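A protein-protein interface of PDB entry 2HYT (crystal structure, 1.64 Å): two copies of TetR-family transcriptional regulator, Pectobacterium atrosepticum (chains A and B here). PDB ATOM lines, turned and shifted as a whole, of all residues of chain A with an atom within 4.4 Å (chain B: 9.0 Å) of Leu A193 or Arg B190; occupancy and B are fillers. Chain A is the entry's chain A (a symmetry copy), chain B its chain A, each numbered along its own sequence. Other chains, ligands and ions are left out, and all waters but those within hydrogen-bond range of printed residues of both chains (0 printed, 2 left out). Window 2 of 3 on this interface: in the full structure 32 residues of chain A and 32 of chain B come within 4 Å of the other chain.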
ATOM      1  N   TRP A  86     -36.903 -12.201   6.674  1.00  0.00           N
ATOM      2  CA  TRP A  86     -36.076 -11.022   6.367  1.00  0.00           C
ATOM      3  C   TRP A  86     -36.921  -9.752   6.414  1.00  0.00           C
ATOM      4  O   TRP A  86     -36.518  -8.742   7.023  1.00  0.00           O
ATOM      5  CB  TRP A  86     -35.415 -11.138   5.003  1.00  0.00           C
ATOM      6  CG  TRP A  86     -34.645  -9.915   4.644  1.00  0.00           C
ATOM      7  CD1 TRP A  86     -34.915  -9.066   3.610  1.00  0.00           C
ATOM      8  CD2 TRP A  86     -33.485  -9.380   5.310  1.00  0.00           C
ATOM      9  NE1 TRP A  86     -34.005  -8.036   3.596  1.00  0.00           N
ATOM     10  CE2 TRP A  86     -33.114  -8.205   4.620  1.00  0.00           C
ATOM     11  CE3 TRP A  86     -32.721  -9.782   6.388  1.00  0.00           C
ATOM     12  CZ2 TRP A  86     -32.008  -7.421   5.005  1.00  0.00           C
ATOM     13  CZ3 TRP A  86     -31.637  -9.006   6.770  1.00  0.00           C
ATOM     14  CH2 TRP A  86     -31.275  -7.855   6.053  1.00  0.00           C
ATOM     15  N   VAL A 144     -30.173 -16.759   5.245  1.00  0.00           N
ATOM     16  CA  VAL A 144     -30.641 -15.456   4.755  1.00  0.00           C
ATOM     17  C   VAL A 144     -29.587 -14.372   4.981  1.00  0.00           C
ATOM     18  O   VAL A 144     -29.301 -13.577   4.065  1.00  0.00           O
ATOM     19  CB  VAL A 144     -32.003 -15.049   5.415  1.00  0.00           C
ATOM     20  CG1 VAL A 144     -32.438 -13.625   5.042  1.00  0.00           C
ATOM     21  CG2 VAL A 144     -33.111 -16.096   5.043  1.00  0.00           C
ATOM     22  N   ALA A 146     -25.657 -13.364   6.041  1.00  0.00           N
ATOM     23  CA  ALA A 146     -24.297 -13.895   5.939  1.00  0.00           C
ATOM     24  C   ALA A 146     -23.688 -14.234   7.305  1.00  0.00           C
ATOM     25  O   ALA A 146     -24.045 -13.654   8.340  1.00  0.00           O
ATOM     26  CB  ALA A 146     -23.376 -12.874   5.184  1.00  0.00           C
ATOM     27  N   LEU A 189     -28.715  -2.287   6.144  1.00  0.00           N
ATOM     28  CA  LEU A 189     -29.211  -3.652   6.338  1.00  0.00           C
ATOM     29  C   LEU A 189     -29.001  -4.509   5.109  1.00  0.00           C
ATOM     30  O   LEU A 189     -28.839  -5.722   5.198  1.00  0.00           O
ATOM     31  CB  LEU A 189     -30.695  -3.639   6.705  1.00  0.00           C
ATOM     32  CG  LEU A 189     -31.050  -2.944   8.023  1.00  0.00           C
ATOM     33  CD1 LEU A 189     -32.533  -3.122   8.300  1.00  0.00           C
ATOM     34  CD2 LEU A 189     -30.209  -3.465   9.217  1.00  0.00           C
ATOM     35  N   ARG A 190     -29.016  -3.912   3.932  1.00  0.00           N
ATOM     36  CA  ARG A 190     -29.011  -4.737   2.733  1.00  0.00           C
ATOM     37  C   ARG A 190     -27.730  -5.563   2.570  1.00  0.00           C
ATOM     38  O   ARG A 190     -27.763  -6.659   1.947  1.00  0.00           O
ATOM     39  CB  ARG A 190     -29.334  -3.891   1.506  1.00  0.00           C
ATOM     40  CG  ARG A 190     -28.198  -3.038   1.043  1.00  0.00           C
ATOM     41  CD  ARG A 190     -28.710  -2.128  -0.059  1.00  0.00           C
ATOM     42  NE  ARG A 190     -27.619  -1.280  -0.541  1.00  0.00           N
ATOM     43  CZ  ARG A 190     -27.687  -0.519  -1.631  1.00  0.00           C
ATOM     44  NH1 ARG A 190     -28.788  -0.488  -2.372  1.00  0.00           N
ATOM     45  NH2 ARG A 190     -26.634   0.206  -1.991  1.00  0.00           N
ATOM     46  N   GLY A 191     -26.634  -5.099   3.176  1.00  0.00           N
ATOM     47  CA  GLY A 191     -25.349  -5.798   3.104  1.00  0.00           C
ATOM     48  C   GLY A 191     -25.334  -7.074   3.920  1.00  0.00           C
ATOM     49  O   GLY A 191     -24.497  -7.944   3.716  1.00  0.00           O
ATOM     50  N   LEU A 192     -26.269  -7.202   4.860  1.00  0.00           N
ATOM     51  CA  LEU A 192     -26.347  -8.439   5.641  1.00  0.00           C
ATOM     52  C   LEU A 192     -26.769  -9.644   4.835  1.00  0.00           C
ATOM     53  O   LEU A 192     -26.493 -10.779   5.254  1.00  0.00           O
ATOM     54  CB  LEU A 192     -27.311  -8.261   6.785  1.00  0.00           C
ATOM     55  CG  LEU A 192     -26.951  -7.091   7.706  1.00  0.00           C
ATOM     56  CD1 LEU A 192     -27.892  -7.158   8.901  1.00  0.00           C
ATOM     57  CD2 LEU A 192     -25.511  -7.096   8.112  1.00  0.00           C
ATOM     58  N   LEU A 193     -27.465  -9.437   3.707  1.00  0.00           N
ATOM     59  CA  LEU A 193     -27.997 -10.553   2.932  1.00  0.00           C
ATOM     60  C   LEU A 193     -26.912 -11.347   2.220  1.00  0.00           C
ATOM     61  O   LEU A 193     -25.942 -10.774   1.707  1.00  0.00           O
ATOM     62  CB  LEU A 193     -28.980 -10.064   1.896  1.00  0.00           C
ATOM     63  CG  LEU A 193     -30.322  -9.541   2.393  1.00  0.00           C
ATOM     64  CD1 LEU A 193     -31.109  -8.793   1.300  1.00  0.00           C
ATOM     65  CD2 LEU A 193     -31.213 -10.691   2.925  1.00  0.00           C
ATOM     66  N   VAL A 194     -27.063 -12.672   2.229  1.00  0.00           N
ATOM     67  CA  VAL A 194     -26.225 -13.546   1.425  1.00  0.00           C
ATOM     68  C   VAL A 194     -26.480 -13.261  -0.067  1.00  0.00           C
ATOM     69  O   VAL A 194     -25.532 -13.073  -0.834  1.00  0.00           O
ATOM     70  CB  VAL A 194     -26.512 -15.034   1.727  1.00  0.00           C
ATOM     71  CG1 VAL A 194     -25.831 -15.944   0.739  1.00  0.00           C
ATOM     72  CG2 VAL A 194     -26.046 -15.365   3.156  1.00  0.00           C
ATOM     73  N   LYS A 195     -27.756 -13.207  -0.427  1.00  0.00           N
ATOM     74  CA  LYS A 195     -28.229 -13.046  -1.798  1.00  0.00           C
ATOM     75  C   LYS A 195     -29.092 -11.779  -1.871  1.00  0.00           C
ATOM     76  O   LYS A 195     -30.130 -11.686  -1.204  1.00  0.00           O
ATOM     77  CB  LYS A 195     -29.076 -14.260  -2.205  1.00  0.00           C
ATOM     78  CG  LYS A 195     -29.693 -14.150  -3.606  1.00  0.00           C
ATOM     79  N   ARG A 197     -31.841  -9.004  -2.884  1.00  0.00           N
ATOM     80  CA  ARG A 197     -33.221  -9.095  -3.331  1.00  0.00           C
ATOM     81  C   ARG A 197     -33.588  -7.920  -4.249  1.00  0.00           C
ATOM     82  O   ARG A 197     -34.599  -7.963  -4.963  1.00  0.00           O
ATOM     83  CB  ARG A 197     -34.136  -9.130  -2.113  1.00  0.00           C
ATOM     84  CG  ARG A 197     -33.812 -10.275  -1.193  1.00  0.00           C
ATOM     85  CD  ARG A 197     -34.906 -10.499  -0.174  1.00  0.00           C
ATOM     86  NE  ARG A 197     -34.640 -11.685   0.640  1.00  0.00           N
ATOM     87  CZ  ARG A 197     -35.482 -12.159   1.549  1.00  0.00           C
ATOM     88  NH1 ARG A 197     -36.653 -11.551   1.775  1.00  0.00           N
ATOM     89  NH2 ARG A 197     -35.158 -13.251   2.232  1.00  0.00           N
ATOM     90  OXT ARG A 197     -32.881  -6.908  -4.307  1.00  0.00           O
ATOM     91  N   TRP B  86     -12.887   5.049   0.343  1.00  0.00           N
ATOM     92  CA  TRP B  86     -13.725   3.984   0.918  1.00  0.00           C
ATOM     93  C   TRP B  86     -12.923   3.157   1.918  1.00  0.00           C
ATOM     94  O   TRP B  86     -13.394   2.877   3.038  1.00  0.00           O
ATOM     95  CB  TRP B  86     -14.289   3.068  -0.157  1.00  0.00           C
ATOM     96  CG  TRP B  86     -15.067   1.937   0.417  1.00  0.00           C
ATOM     97  CD1 TRP B  86     -14.752   0.612   0.328  1.00  0.00           C
ATOM     98  CD2 TRP B  86     -16.284   2.007   1.185  1.00  0.00           C
ATOM     99  NE1 TRP B  86     -15.688  -0.142   0.994  1.00  0.00           N
ATOM    100  CE2 TRP B  86     -16.641   0.684   1.523  1.00  0.00           C
ATOM    101  CE3 TRP B  86     -17.108   3.038   1.593  1.00  0.00           C
ATOM    102  CZ2 TRP B  86     -17.793   0.381   2.276  1.00  0.00           C
ATOM    103  CZ3 TRP B  86     -18.237   2.739   2.341  1.00  0.00           C
ATOM    104  CH2 TRP B  86     -18.582   1.413   2.643  1.00  0.00           C
ATOM    105  N   PHE B  89     -12.448   5.025   5.076  1.00  0.00           N
ATOM    106  CA  PHE B  89     -13.664   5.003   5.898  1.00  0.00           C
ATOM    107  C   PHE B  89     -13.764   3.678   6.651  1.00  0.00           C
ATOM    108  O   PHE B  89     -14.033   3.682   7.852  1.00  0.00           O
ATOM    109  CB  PHE B  89     -14.888   5.236   4.985  1.00  0.00           C
ATOM    110  CG  PHE B  89     -16.187   4.781   5.587  1.00  0.00           C
ATOM    111  CD1 PHE B  89     -16.820   5.546   6.500  1.00  0.00           C
ATOM    112  CD2 PHE B  89     -16.776   3.585   5.198  1.00  0.00           C
ATOM    113  CE1 PHE B  89     -18.039   5.142   7.042  1.00  0.00           C
ATOM    114  CE2 PHE B  89     -17.980   3.184   5.720  1.00  0.00           C
ATOM    115  CZ  PHE B  89     -18.618   3.973   6.667  1.00  0.00           C
ATOM    116  N   ARG B  90     -13.529   2.558   5.971  1.00  0.00           N
ATOM    117  CA  ARG B  90     -13.519   1.223   6.648  1.00  0.00           C
ATOM    118  C   ARG B  90     -12.466   1.220   7.736  1.00  0.00           C
ATOM    119  O   ARG B  90     -12.706   0.730   8.836  1.00  0.00           O
ATOM    120  CB  ARG B  90     -13.235   0.094   5.663  1.00  0.00           C
ATOM    121  CG  ARG B  90     -14.394  -0.149   4.686  1.00  0.00           C
ATOM    122  CD  ARG B  90     -14.080  -1.280   3.673  1.00  0.00           C
ATOM    123  NE  ARG B  90     -13.536  -2.472   4.297  1.00  0.00           N
ATOM    124  CZ  ARG B  90     -12.746  -3.365   3.712  1.00  0.00           C
ATOM    125  NH1 ARG B  90     -12.396  -3.238   2.439  1.00  0.00           N
ATOM    126  NH2 ARG B  90     -12.301  -4.400   4.414  1.00  0.00           N
ATOM    127  N   VAL B 144     -19.370   7.009  -4.373  1.00  0.00           N
ATOM    128  CA  VAL B 144     -18.908   5.763  -3.747  1.00  0.00           C
ATOM    129  C   VAL B 144     -20.006   5.139  -2.885  1.00  0.00           C
ATOM    130  O   VAL B 144     -20.251   3.920  -2.971  1.00  0.00           O
ATOM    131  CB  VAL B 144     -17.607   5.992  -2.905  1.00  0.00           C
ATOM    132  CG1 VAL B 144     -17.188   4.744  -2.114  1.00  0.00           C
ATOM    133  CG2 VAL B 144     -16.446   6.486  -3.837  1.00  0.00           C
ATOM    134  N   VAL B 145     -20.637   5.974  -2.057  1.00  0.00           N
ATOM    135  CA  VAL B 145     -21.725   5.582  -1.152  1.00  0.00           C
ATOM    136  C   VAL B 145     -23.058   6.001  -1.760  1.00  0.00           C
ATOM    137  O   VAL B 145     -23.215   7.102  -2.305  1.00  0.00           O
ATOM    138  CB  VAL B 145     -21.511   6.140   0.264  1.00  0.00           C
ATOM    139  CG1 VAL B 145     -22.828   6.076   1.185  1.00  0.00           C
ATOM    140  CG2 VAL B 145     -20.347   5.414   0.927  1.00  0.00           C
ATOM    141  N   ALA B 146     -24.026   5.082  -1.695  1.00  0.00           N
ATOM    142  CA  ALA B 146     -25.360   5.340  -2.238  1.00  0.00           C
ATOM    143  C   ALA B 146     -26.051   6.538  -1.574  1.00  0.00           C
ATOM    144  O   ALA B 146     -25.782   6.885  -0.416  1.00  0.00           O
ATOM    145  CB  ALA B 146     -26.257   4.061  -2.094  1.00  0.00           C
ATOM    146  N   ALA B 183     -15.615  -8.154  11.836  1.00  0.00           N
ATOM    147  CA  ALA B 183     -16.181  -8.968  10.746  1.00  0.00           C
ATOM    148  C   ALA B 183     -17.643  -8.627  10.532  1.00  0.00           C
ATOM    149  O   ALA B 183     -18.102  -8.575   9.408  1.00  0.00           O
ATOM    150  CB  ALA B 183     -16.012 -10.463  11.019  1.00  0.00           C
ATOM    151  N   ALA B 184     -18.399  -8.454  11.618  1.00  0.00           N
ATOM    152  CA  ALA B 184     -19.834  -8.133  11.484  1.00  0.00           C
ATOM    153  C   ALA B 184     -19.981  -6.722  10.869  1.00  0.00           C
ATOM    154  O   ALA B 184     -20.817  -6.476  10.009  1.00  0.00           O
ATOM    155  CB  ALA B 184     -20.504  -8.212  12.838  1.00  0.00           C
ATOM    156  N   LEU B 185     -19.159  -5.796  11.351  1.00  0.00           N
ATOM    157  CA  LEU B 185     -19.179  -4.421  10.842  1.00  0.00           C
ATOM    158  C   LEU B 185     -19.034  -4.389   9.313  1.00  0.00           C
ATOM    159  O   LEU B 185     -19.722  -3.627   8.606  1.00  0.00           O
ATOM    160  CB  LEU B 185     -18.070  -3.625  11.500  1.00  0.00           C
ATOM    161  CG  LEU B 185     -17.850  -2.201  10.993  1.00  0.00           C
ATOM    162  CD1 LEU B 185     -19.050  -1.295  11.313  1.00  0.00           C
ATOM    163  CD2 LEU B 185     -16.556  -1.652  11.632  1.00  0.00           C
ATOM    164  N   GLU B 186     -18.119  -5.197   8.803  1.00  0.00           N
ATOM    165  CA  GLU B 186     -17.862  -5.231   7.365  1.00  0.00           C
ATOM    166  C   GLU B 186     -19.127  -5.592   6.574  1.00  0.00           C
ATOM    167  O   GLU B 186     -19.354  -5.064   5.495  1.00  0.00           O
ATOM    168  CB  GLU B 186     -16.710  -6.178   7.008  1.00  0.00           C
ATOM    169  CG  GLU B 186     -15.351  -5.782   7.578  1.00  0.00           C
ATOM    170  CD  GLU B 186     -14.697  -4.556   6.937  1.00  0.00           C
ATOM    171  OE1 GLU B 186     -15.340  -3.771   6.189  1.00  0.00           O
ATOM    172  OE2 GLU B 186     -13.492  -4.372   7.230  1.00  0.00           O
ATOM    173  N   LEU B 187     -19.970  -6.488   7.108  1.00  0.00           N
ATOM    174  CA  LEU B 187     -21.231  -6.823   6.460  1.00  0.00           C
ATOM    175  C   LEU B 187     -22.192  -5.654   6.462  1.00  0.00           C
ATOM    176  O   LEU B 187     -22.920  -5.421   5.504  1.00  0.00           O
ATOM    177  CB  LEU B 187     -21.924  -7.994   7.174  1.00  0.00           C
ATOM    178  CG  LEU B 187     -21.205  -9.318   7.102  1.00  0.00           C
ATOM    179  CD1 LEU B 187     -22.065 -10.281   7.956  1.00  0.00           C
ATOM    180  CD2 LEU B 187     -21.053  -9.804   5.636  1.00  0.00           C
ATOM    181  N   LEU B 188     -22.248  -4.924   7.565  1.00  0.00           N
ATOM    182  CA  LEU B 188     -23.093  -3.725   7.561  1.00  0.00           C
ATOM    183  C   LEU B 188     -22.605  -2.658   6.598  1.00  0.00           C
ATOM    184  O   LEU B 188     -23.391  -1.975   5.928  1.00  0.00           O
ATOM    185  CB  LEU B 188     -23.161  -3.093   8.928  1.00  0.00           C
ATOM    186  CG  LEU B 188     -24.143  -3.652   9.939  1.00  0.00           C
ATOM    187  CD1 LEU B 188     -24.054  -2.765  11.149  1.00  0.00           C
ATOM    188  CD2 LEU B 188     -25.579  -3.719   9.382  1.00  0.00           C
ATOM    189  N   LEU B 189     -21.303  -2.475   6.522  1.00  0.00           N
ATOM    190  CA  LEU B 189     -20.782  -1.371   5.712  1.00  0.00           C
ATOM    191  C   LEU B 189     -20.883  -1.661   4.230  1.00  0.00           C
ATOM    192  O   LEU B 189     -21.016  -0.756   3.412  1.00  0.00           O
ATOM    193  CB  LEU B 189     -19.327  -1.075   6.077  1.00  0.00           C
ATOM    194  CG  LEU B 189     -19.082  -0.605   7.513  1.00  0.00           C
ATOM    195  CD1 LEU B 189     -17.618  -0.239   7.679  1.00  0.00           C
ATOM    196  CD2 LEU B 189     -19.987   0.590   7.913  1.00  0.00           C
ATOM    197  N   ARG B 190     -20.804  -2.919   3.842  1.00  0.00           N
ATOM    198  CA  ARG B 190     -20.705  -3.204   2.418  1.00  0.00           C
ATOM    199  C   ARG B 190     -21.947  -2.781   1.626  1.00  0.00           C
ATOM    200  O   ARG B 190     -21.840  -2.464   0.410  1.00  0.00           O
ATOM    201  CB  ARG B 190     -20.323  -4.664   2.194  1.00  0.00           C
ATOM    202  CG  ARG B 190     -21.449  -5.622   2.408  1.00  0.00           C
ATOM    203  CD  ARG B 190     -20.889  -7.031   2.329  1.00  0.00           C
ATOM    204  NE  ARG B 190     -21.970  -8.000   2.527  1.00  0.00           N
ATOM    205  CZ  ARG B 190     -21.850  -9.308   2.320  1.00  0.00           C
ATOM    206  NH1 ARG B 190     -20.701  -9.829   1.903  1.00  0.00           N
ATOM    207  NH2 ARG B 190     -22.895 -10.102   2.519  1.00  0.00           N
ATOM    208  N   GLY B 191     -23.095  -2.703   2.304  1.00  0.00           N
ATOM    209  CA  GLY B 191     -24.351  -2.304   1.666  1.00  0.00           C
ATOM    210  C   GLY B 191     -24.385  -0.830   1.318  1.00  0.00           C
ATOM    211  O   GLY B 191     -25.181  -0.394   0.496  1.00  0.00           O
ATOM    212  N   LEU B 192     -23.513  -0.040   1.943  1.00  0.00           N
ATOM    213  CA  LEU B 192     -23.453   1.384   1.603  1.00  0.00           C
ATOM    214  C   LEU B 192     -22.942   1.658   0.209  1.00  0.00           C
ATOM    215  O   LEU B 192     -23.213   2.742  -0.332  1.00  0.00           O
ATOM    216  CB  LEU B 192     -22.574   2.107   2.591  1.00  0.00           C
ATOM    217  CG  LEU B 192     -23.029   1.941   4.043  1.00  0.00           C
ATOM    218  CD1 LEU B 192     -22.171   2.871   4.890  1.00  0.00           C
ATOM    219  CD2 LEU B 192     -24.493   2.194   4.224  1.00  0.00           C
ATOM    220  N   LEU B 193     -22.177   0.726  -0.379  1.00  0.00           N
ATOM    221  CA  LEU B 193     -21.562   0.963  -1.681  1.00  0.00           C
ATOM    222  C   LEU B 193     -22.573   0.975  -2.817  1.00  0.00           C
ATOM    223  O   LEU B 193     -23.521   0.180  -2.829  1.00  0.00           O
ATOM    224  CB  LEU B 193     -20.525  -0.092  -1.983  1.00  0.00           C
ATOM    225  CG  LEU B 193     -19.236  -0.061  -1.170  1.00  0.00           C
ATOM    226  CD1 LEU B 193     -18.398  -1.343  -1.341  1.00  0.00           C
ATOM    227  CD2 LEU B 193     -18.350   1.146  -1.564  1.00  0.00           C
ATOM    228  N   VAL B 194     -22.384   1.909  -3.750  1.00  0.00           N
ATOM    229  CA  VAL B 194     -23.141   1.918  -4.991  1.00  0.00           C
ATOM    230  C   VAL B 194     -22.793   0.658  -5.805  1.00  0.00           C
ATOM    231  O   VAL B 194     -23.692  -0.050  -6.268  1.00  0.00           O
ATOM    232  CB  VAL B 194     -22.831   3.181  -5.828  1.00  0.00           C
ATOM    233  CG1 VAL B 194     -23.417   3.087  -7.213  1.00  0.00           C
ATOM    234  CG2 VAL B 194     -23.384   4.422  -5.105  1.00  0.00           C
ATOM    235  N   LYS B 195     -21.497   0.399  -5.930  1.00  0.00           N
ATOM    236  CA  LYS B 195     -20.936  -0.681  -6.733  1.00  0.00           C
ATOM    237  C   LYS B 195     -20.107  -1.592  -5.818  1.00  0.00           C
ATOM    238  O   LYS B 195     -19.120  -1.150  -5.218  1.00  0.00           O
ATOM    239  CB  LYS B 195     -20.030  -0.102  -7.829  1.00  0.00           C
ATOM    240  CG  LYS B 195     -19.322  -1.165  -8.681  1.00  0.00           C
ATOM    241  N   PRO B 196     -20.503  -2.869  -5.688  1.00  0.00           N
ATOM    242  CA  PRO B 196     -19.710  -3.769  -4.836  1.00  0.00           C
ATOM    243  C   PRO B 196     -18.270  -3.921  -5.299  1.00  0.00           C
ATOM    244  O   PRO B 196     -17.987  -3.830  -6.498  1.00  0.00           O
ATOM    245  CB  PRO B 196     -20.438  -5.116  -4.963  1.00  0.00           C
ATOM    246  CG  PRO B 196     -21.851  -4.759  -5.398  1.00  0.00           C
ATOM    247  CD  PRO B 196     -21.666  -3.549  -6.289  1.00  0.00           C
ATOM    248  N   ARG B 197     -17.378  -4.173  -4.346  1.00  0.00           N
ATOM    249  CA  ARG B 197     -15.968  -4.389  -4.627  1.00  0.00           C
ATOM    250  C   ARG B 197     -15.573  -5.857  -4.398  1.00  0.00           C
ATOM    251  O   ARG B 197     -14.515  -6.308  -4.857  1.00  0.00           O
ATOM    252  CB  ARG B 197     -15.137  -3.467  -3.745  1.00  0.00           C
ATOM    253  CG  ARG B 197     -15.490  -2.019  -3.949  1.00  0.00           C
ATOM    254  CD  ARG B 197     -14.462  -1.101  -3.328  1.00  0.00           C
ATOM    255  NE  ARG B 197     -14.748   0.301  -3.630  1.00  0.00           N
ATOM    256  CZ  ARG B 197     -13.957   1.307  -3.282  1.00  0.00           C
ATOM    257  NH1 ARG B 197     -12.822   1.079  -2.609  1.00  0.00           N
ATOM    258  NH2 ARG B 197     -14.296   2.548  -3.612  1.00  0.00           N
ATOM    259  OXT ARG B 197     -16.304  -6.624  -3.761  1.00  0.00           O
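NE of Arg B190 lies within hydrogen-bond range of O of Gly A191, 2.8 Å away.
O of Leu A193 sits at hydrogen-bond distance from NH2 of Arg B190 (3.2 Å).
NE of Arg A190 is in hydrogen-bond range of O of Gly B191, 2.8 Å away.
O of Leu B193 is in hydrogen-bond range of NH2 of Arg A190 (3.2 Å).
O of Leu B187 sits close to O of Gly A191.
N of Ala B146 lies within hydrogen-bond range of O of Leu B192.
The backbone carbonyl oxygen of Leu A192 is in hydrogen-bond range of the backbone NH of Ala A146 (2.8 Å).
Among the printed residues, pairs that only touch across the chains: Leu A192 with Leu B188, Leu A192 with Leu B187, Arg A190 with Ala B146, Ala A146 with Arg B190, Ala A146 with Leu B187 and Gly A191 with Gly B191.
Of chain B, only Arg B190 (3.2 Å) comes within 4 Å of Leu A193.
Arg B190 touches just these residues of chain A: Ala A146 (3.9 Å), Gly A191 (2.8 Å) and Leu A193 (3.2 Å).
Gly A191 touches just these residues of chain B: Leu B187, Arg B190 and Gly B191.
No residue of chain B comes within 4 Å of Val A194.
Printed residues of chain A within 4 Å of Leu B188: Leu A192.
Printed residues of chain A within 4 Å of Leu B193: Arg A190 (3.2 Å).
Of the printed residues of chain B, Arg A190 touches Ala B146 (3.9 Å), Gly B191 (2.8 Å) and Leu B193 (3.2 Å).
The nearest residue of chain B that does not touch Leu A193 is Leu B187 (6.3 Å).
The nearest printed residue of chain B that does not touch Arg A190 is Leu B192 (4.5 Å).
Of the 21 printed residues of chain B, 6 touch a printed residue of chain A.
Hydrophobic or aromatic side chains of chain B that line the printed part of chain A: Ala B146, Leu B187 and Leu B188.
Printed residues of chain A that touch a printed residue of chain B: Ala A146, Arg A190, Gly A191, Leu A192 and Leu A193.
Hydrophobic or aromatic side chains of chain A within 4 Å of the printed part of chain B: Ala A146 and Leu A192.
Among the printed residues, no Asp or Glu carboxylate lies within 4 Å of a Lys or Arg side-chain nitrogen of the other chain.
Ala A146 touches Arg B190, and with the chains exchanged Arg A190 touches Ala B146.
Arg A190 touches Gly B191, and with the chains exchanged Gly A191 touches Arg B190.
Arg A190 touches Leu B193, and with the chains exchanged Leu A193 touches Arg B190.
Gly B191 touches its own counterpart, Gly A191.
Positions printed for both chains: 86, 144, 146, 189, 190, 191, 192, 193, 194, 195 and 197.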
